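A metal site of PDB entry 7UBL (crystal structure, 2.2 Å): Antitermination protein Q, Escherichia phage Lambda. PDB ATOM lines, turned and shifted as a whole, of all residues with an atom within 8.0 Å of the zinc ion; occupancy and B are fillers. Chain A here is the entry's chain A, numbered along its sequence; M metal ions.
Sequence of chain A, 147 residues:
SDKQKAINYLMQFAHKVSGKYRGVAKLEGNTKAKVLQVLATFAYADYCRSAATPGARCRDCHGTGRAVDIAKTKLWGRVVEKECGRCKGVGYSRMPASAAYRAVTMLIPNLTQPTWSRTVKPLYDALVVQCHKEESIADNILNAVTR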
ATOM      1  N   ALA A  56      19.909 -31.137  21.707  1.00  0.00           N
ATOM      2  CA  ALA A  56      19.655 -29.848  22.350  1.00  0.00           C
ATOM      3  C   ALA A  56      20.461 -28.697  21.773  1.00  0.00           C
ATOM      4  O   ALA A  56      20.055 -27.534  21.942  1.00  0.00           O
ATOM      5  CB  ALA A  56      19.964 -29.956  23.853  1.00  0.00           C
ATOM      6  N   ARG A  57      21.565 -28.961  21.088  1.00  0.00           N
ATOM      7  CA  ARG A  57      22.502 -27.898  20.736  1.00  0.00           C
ATOM      8  C   ARG A  57      21.902 -26.936  19.715  1.00  0.00           C
ATOM      9  O   ARG A  57      21.395 -27.362  18.666  1.00  0.00           O
ATOM     10  CB  ARG A  57      23.793 -28.489  20.176  1.00  0.00           C
ATOM     11  CG  ARG A  57      24.807 -27.442  19.718  1.00  0.00           C
ATOM     12  CD  ARG A  57      26.112 -28.058  19.247  1.00  0.00           C
ATOM     13  NE  ARG A  57      27.061 -28.199  20.346  1.00  0.00           N
ATOM     14  CZ  ARG A  57      27.364 -29.344  20.953  1.00  0.00           C
ATOM     15  NH1 ARG A  57      26.797 -30.487  20.590  1.00  0.00           N
ATOM     16  NH2 ARG A  57      28.236 -29.341  21.942  1.00  0.00           N
ATOM     17  N   CYS A  58      21.981 -25.636  19.996  1.00  0.00           N
ATOM     18  CA  CYS A  58      21.447 -24.641  19.074  1.00  0.00           C
ATOM     19  C   CYS A  58      22.111 -24.763  17.702  1.00  0.00           C
ATOM     20  O   CYS A  58      23.340 -24.807  17.591  1.00  0.00           O
ATOM     21  CB  CYS A  58      21.645 -23.223  19.614  1.00  0.00           C
ATOM     22  SG  CYS A  58      21.109 -21.906  18.452  1.00  0.00           S
ATOM     23  N   ARG A  59      21.289 -24.786  16.662  1.00  0.00           N
ATOM     24  CA  ARG A  59      21.774 -24.996  15.308  1.00  0.00           C
ATOM     25  C   ARG A  59      22.512 -23.774  14.768  1.00  0.00           C
ATOM     26  O   ARG A  59      23.378 -23.914  13.908  1.00  0.00           O
ATOM     27  CB  ARG A  59      20.588 -25.349  14.404  1.00  0.00           C
ATOM     28  CG  ARG A  59      20.930 -25.569  12.938  1.00  0.00           C
ATOM     29  CD  ARG A  59      19.680 -25.457  12.090  1.00  0.00           C
ATOM     30  NE  ARG A  59      19.223 -24.075  11.990  1.00  0.00           N
ATOM     31  CZ  ARG A  59      18.099 -23.699  11.389  1.00  0.00           C
ATOM     32  NH1 ARG A  59      17.295 -24.604  10.838  1.00  0.00           N
ATOM     33  NH2 ARG A  59      17.770 -22.411  11.348  1.00  0.00           N
ATOM     34  N   ASP A  60      22.169 -22.576  15.246  1.00  0.00           N
ATOM     35  CA  ASP A  60      22.737 -21.366  14.649  1.00  0.00           C
ATOM     36  C   ASP A  60      24.058 -20.962  15.287  1.00  0.00           C
ATOM     37  O   ASP A  60      24.942 -20.480  14.588  1.00  0.00           O
ATOM     38  CB  ASP A  60      21.725 -20.214  14.752  1.00  0.00           C
ATOM     39  CG  ASP A  60      20.679 -20.268  13.655  1.00  0.00           C
ATOM     40  OD1 ASP A  60      20.712 -21.218  12.835  1.00  0.00           O
ATOM     41  OD2 ASP A  60      19.828 -19.356  13.608  1.00  0.00           O
ATOM     42  N   CYS A  61      24.214 -21.134  16.601  1.00  0.00           N
ATOM     43  CA  CYS A  61      25.448 -20.784  17.294  1.00  0.00           C
ATOM     44  C   CYS A  61      26.283 -21.991  17.701  1.00  0.00           C
ATOM     45  O   CYS A  61      27.377 -21.809  18.234  1.00  0.00           O
ATOM     46  CB  CYS A  61      25.137 -19.927  18.528  1.00  0.00           C
ATOM     47  SG  CYS A  61      24.253 -20.816  19.839  1.00  0.00           S
ATOM     48  N   HIS A  62      25.783 -23.204  17.479  1.00  0.00           N
ATOM     49  CA  HIS A  62      26.501 -24.432  17.817  1.00  0.00           C
ATOM     50  C   HIS A  62      26.894 -24.488  19.288  1.00  0.00           C
ATOM     51  O   HIS A  62      27.867 -25.158  19.652  1.00  0.00           O
ATOM     52  CB  HIS A  62      27.732 -24.606  16.929  1.00  0.00           C
ATOM     53  CG  HIS A  62      27.430 -24.479  15.462  1.00  0.00           C
ATOM     54  ND1 HIS A  62      27.990 -23.491  14.680  1.00  0.00           N
ATOM     55  CD2 HIS A  62      26.625 -25.197  14.657  1.00  0.00           C
ATOM     56  CE1 HIS A  62      27.548 -23.613  13.443  1.00  0.00           C
ATOM     57  NE2 HIS A  62      26.714 -24.639  13.400  1.00  0.00           N
ATOM     58  N   GLY A  63      26.147 -23.818  20.161  1.00  0.00           N
ATOM     59  CA  GLY A  63      26.317 -23.946  21.597  1.00  0.00           C
ATOM     60  C   GLY A  63      26.974 -22.757  22.274  1.00  0.00           C
ATOM     61  O   GLY A  63      26.949 -22.696  23.512  1.00  0.00           O
ATOM     62  N   THR A  64      27.548 -21.827  21.518  1.00  0.00           N
ATOM     63  CA  THR A  64      28.192 -20.669  22.153  1.00  0.00           C
ATOM     64  C   THR A  64      27.178 -19.703  22.719  1.00  0.00           C
ATOM     65  O   THR A  64      27.491 -18.943  23.653  1.00  0.00           O
ATOM     66  CB  THR A  64      29.086 -19.941  21.151  1.00  0.00           C
ATOM     67  OG1 THR A  64      28.262 -19.387  20.109  1.00  0.00           O
ATOM     68  CG2 THR A  64      30.110 -20.896  20.529  1.00  0.00           C
ATOM     69  N   GLY A  65      25.961 -19.683  22.178  1.00  0.00           N
ATOM     70  CA  GLY A  65      24.976 -18.685  22.564  1.00  0.00           C
ATOM     71  C   GLY A  65      25.308 -17.273  22.134  1.00  0.00           C
ATOM     72  O   GLY A  65      24.726 -16.322  22.662  1.00  0.00           O
ATOM     73  N   ARG A  66      26.236 -17.100  21.178  1.00  0.00           N
ATOM     74  CA  ARG A  66      26.689 -15.780  20.766  1.00  0.00           C
ATOM     75  C   ARG A  66      26.626 -15.628  19.252  1.00  0.00           C
ATOM     76  O   ARG A  66      26.753 -16.603  18.505  1.00  0.00           O
ATOM     77  CB  ARG A  66      28.130 -15.517  21.239  1.00  0.00           C
ATOM     78  CG  ARG A  66      28.283 -15.396  22.759  1.00  0.00           C
ATOM     79  CD  ARG A  66      27.337 -14.340  23.314  1.00  0.00           C
ATOM     80  NE  ARG A  66      27.884 -13.659  24.483  1.00  0.00           N
ATOM     81  CZ  ARG A  66      27.564 -12.411  24.830  1.00  0.00           C
ATOM     82  NH1 ARG A  66      26.702 -11.706  24.113  1.00  0.00           N
ATOM     83  NH2 ARG A  66      28.112 -11.876  25.917  1.00  0.00           N
ATOM     84  N   ALA A  67      26.412 -14.393  18.811  1.00  0.00           N
ATOM     85  CA  ALA A  67      26.386 -14.089  17.386  1.00  0.00           C
ATOM     86  C   ALA A  67      26.710 -12.614  17.200  1.00  0.00           C
ATOM     87  O   ALA A  67      26.316 -11.782  18.019  1.00  0.00           O
ATOM     88  CB  ALA A  67      25.027 -14.412  16.758  1.00  0.00           C
ATOM     89  N   GLU A  83      23.597 -11.851  22.194  1.00  0.00           N
ATOM     90  CA  GLU A  83      23.042 -13.177  22.428  1.00  0.00           C
ATOM     91  C   GLU A  83      22.493 -13.746  21.131  1.00  0.00           C
ATOM     92  O   GLU A  83      21.833 -13.047  20.359  1.00  0.00           O
ATOM     93  CB  GLU A  83      21.927 -13.130  23.469  1.00  0.00           C
ATOM     94  CG  GLU A  83      22.390 -12.766  24.864  1.00  0.00           C
ATOM     95  CD  GLU A  83      21.271 -12.863  25.886  1.00  0.00           C
ATOM     96  OE1 GLU A  83      20.089 -12.756  25.483  1.00  0.00           O
ATOM     97  OE2 GLU A  83      21.562 -13.053  27.080  1.00  0.00           O
ATOM     98  N   CYS A  84      22.779 -15.024  20.890  1.00  0.00           N
ATOM     99  CA  CYS A  84      22.232 -15.683  19.714  1.00  0.00           C
ATOM    100  C   CYS A  84      20.710 -15.610  19.734  1.00  0.00           C
ATOM    101  O   CYS A  84      20.067 -15.995  20.711  1.00  0.00           O
ATOM    102  CB  CYS A  84      22.703 -17.147  19.660  1.00  0.00           C
ATOM    103  SG  CYS A  84      21.799 -18.120  18.467  1.00  0.00           S
ATOM    104  N   GLY A  85      20.141 -15.113  18.638  1.00  0.00           N
ATOM    105  CA  GLY A  85      18.711 -14.889  18.585  1.00  0.00           C
ATOM    106  C   GLY A  85      17.880 -16.163  18.647  1.00  0.00           C
ATOM    107  O   GLY A  85      16.779 -16.160  19.188  1.00  0.00           O
ATOM    108  N   ARG A  86      18.394 -17.256  18.083  1.00  0.00           N
ATOM    109  CA  ARG A  86      17.604 -18.471  17.998  1.00  0.00           C
ATOM    110  C   ARG A  86      17.445 -19.132  19.365  1.00  0.00           C
ATOM    111  O   ARG A  86      16.372 -19.643  19.679  1.00  0.00           O
ATOM    112  CB  ARG A  86      18.252 -19.444  17.013  1.00  0.00           C
ATOM    113  CG  ARG A  86      17.398 -20.678  16.740  1.00  0.00           C
ATOM    114  CD  ARG A  86      17.992 -21.531  15.640  1.00  0.00           C
ATOM    115  NE  ARG A  86      17.132 -22.672  15.319  1.00  0.00           N
ATOM    116  CZ  ARG A  86      16.172 -22.662  14.406  1.00  0.00           C
ATOM    117  NH1 ARG A  86      15.927 -21.574  13.686  1.00  0.00           N
ATOM    118  NH2 ARG A  86      15.451 -23.755  14.196  1.00  0.00           N
ATOM    119  N   CYS A  87      18.505 -19.135  20.174  1.00  0.00           N
ATOM    120  CA  CYS A  87      18.499 -19.767  21.479  1.00  0.00           C
ATOM    121  C   CYS A  87      18.485 -18.758  22.614  1.00  0.00           C
ATOM    122  O   CYS A  87      18.666 -19.149  23.771  1.00  0.00           O
ATOM    123  CB  CYS A  87      19.709 -20.685  21.647  1.00  0.00           C
ATOM    124  SG  CYS A  87      21.257 -19.773  21.868  1.00  0.00           S
ATOM    125  N   LYS A  88      18.308 -17.474  22.303  1.00  0.00           N
ATOM    126  CA  LYS A  88      18.269 -16.420  23.322  1.00  0.00           C
ATOM    127  C   LYS A  88      19.463 -16.518  24.265  1.00  0.00           C
ATOM    128  O   LYS A  88      19.350 -16.257  25.471  1.00  0.00           O
ATOM    129  CB  LYS A  88      16.935 -16.450  24.069  1.00  0.00           C
ATOM    130  CG  LYS A  88      15.748 -16.292  23.140  1.00  0.00           C
ATOM    131  CD  LYS A  88      14.428 -16.207  23.863  1.00  0.00           C
ATOM    132  CE  LYS A  88      13.319 -15.902  22.864  1.00  0.00           C
ATOM    133  NZ  LYS A  88      12.011 -15.602  23.511  1.00  0.00           N
ATOM    134  N   GLY A  89      20.615 -16.889  23.723  1.00  0.00           N
ATOM    135  CA  GLY A  89      21.868 -16.832  24.448  1.00  0.00           C
ATOM    136  C   GLY A  89      22.200 -18.046  25.282  1.00  0.00           C
ATOM    137  O   GLY A  89      23.282 -18.079  25.889  1.00  0.00           O
ATOM    138  N   VAL A  90      21.324 -19.054  25.330  1.00  0.00           N
ATOM    139  CA  VAL A  90      21.576 -20.224  26.168  1.00  0.00           C
ATOM    140  C   VAL A  90      22.532 -21.189  25.481  1.00  0.00           C
ATOM    141  O   VAL A  90      23.347 -21.838  26.154  1.00  0.00           O
ATOM    142  CB  VAL A  90      20.242 -20.917  26.514  1.00  0.00           C
ATOM    143  CG1 VAL A  90      20.483 -22.148  27.401  1.00  0.00           C
ATOM    144  CG2 VAL A  90      19.294 -19.936  27.195  1.00  0.00           C
ATOM    145  N   GLY A  91      22.451 -21.317  24.156  1.00  0.00           N
ATOM    146  CA  GLY A  91      23.256 -22.276  23.426  1.00  0.00           C
ATOM    147  C   GLY A  91      22.613 -23.635  23.247  1.00  0.00           C
ATOM    148  O   GLY A  91      23.162 -24.478  22.534  1.00  0.00           O
ATOM    149  N   TYR A  92      21.474 -23.874  23.884  1.00  0.00           N
ATOM    150  CA  TYR A  92      20.793 -25.162  23.791  1.00  0.00           C
ATOM    151  C   TYR A  92      19.355 -24.954  24.204  1.00  0.00           C
ATOM    152  O   TYR A  92      19.016 -23.970  24.860  1.00  0.00           O
ATOM    153  CB  TYR A  92      21.466 -26.224  24.659  1.00  0.00           C
ATOM    154  CG  TYR A  92      21.477 -25.858  26.129  1.00  0.00           C
ATOM    155  CD1 TYR A  92      22.534 -25.142  26.685  1.00  0.00           C
ATOM    156  CD2 TYR A  92      20.417 -26.225  26.964  1.00  0.00           C
ATOM    157  CE1 TYR A  92      22.539 -24.803  28.027  1.00  0.00           C
ATOM    158  CE2 TYR A  92      20.422 -25.886  28.307  1.00  0.00           C
ATOM    159  CZ  TYR A  92      21.490 -25.175  28.832  1.00  0.00           C
ATOM    160  OH  TYR A  92      21.496 -24.836  30.174  1.00  0.00           O
ATOM    161  N   SER A  93      18.504 -25.909  23.818  1.00  0.00           N
ATOM    162  CA  SER A  93      17.085 -25.816  24.095  1.00  0.00           C
ATOM    163  C   SER A  93      16.740 -26.402  25.464  1.00  0.00           C
ATOM    164  O   SER A  93      17.392 -27.337  25.941  1.00  0.00           O
ATOM    165  CB  SER A  93      16.280 -26.552  23.024  1.00  0.00           C
ATOM    166  OG  SER A  93      16.661 -27.910  22.936  1.00  0.00           O
HETATM  167 ZN    ZN M   1      22.043 -20.211  19.566  1.00  0.00          ZN
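The backbone carbonyl oxygen (O) of Gly 91 sits at hydrogen-bond distance from the backbone NH (N) of Cys 58. The backbone carbonyl oxygen (O) of Cys 61 sits at hydrogen-bond distance from the side-chain hydroxyl (OG1) of Thr 64. The backbone NH of Cys 84 lies within hydrogen-bond range of the backbone carbonyl oxygen of Gly 65, 2.9 Å away. The backbone NH of Gly 89 sits at hydrogen-bond distance from the backbone carbonyl oxygen of Cys 84, 3.2 Å away. N of Gly 63 sits close to SG of Cys 61. The side-chain sulfur (SG) of Cys 87 lies close to the backbone NH (N) of Val 90, at 3.5 Å. N of Asp 60 lies close to SG of Cys 58 (3.4 Å). N of Gly 89 sits close to SG of Cys 87 (3.5 Å).
The zinc ion is bound by the side-chain sulfur (SG) of Cys 58 (2.2 Å), the side-chain sulfur (SG) of Cys 61 (2.3 Å), the side-chain sulfur (SG) of Cys 84 (2.4 Å) and the side-chain sulfur (SG) of Cys 87 (2.5 Å).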
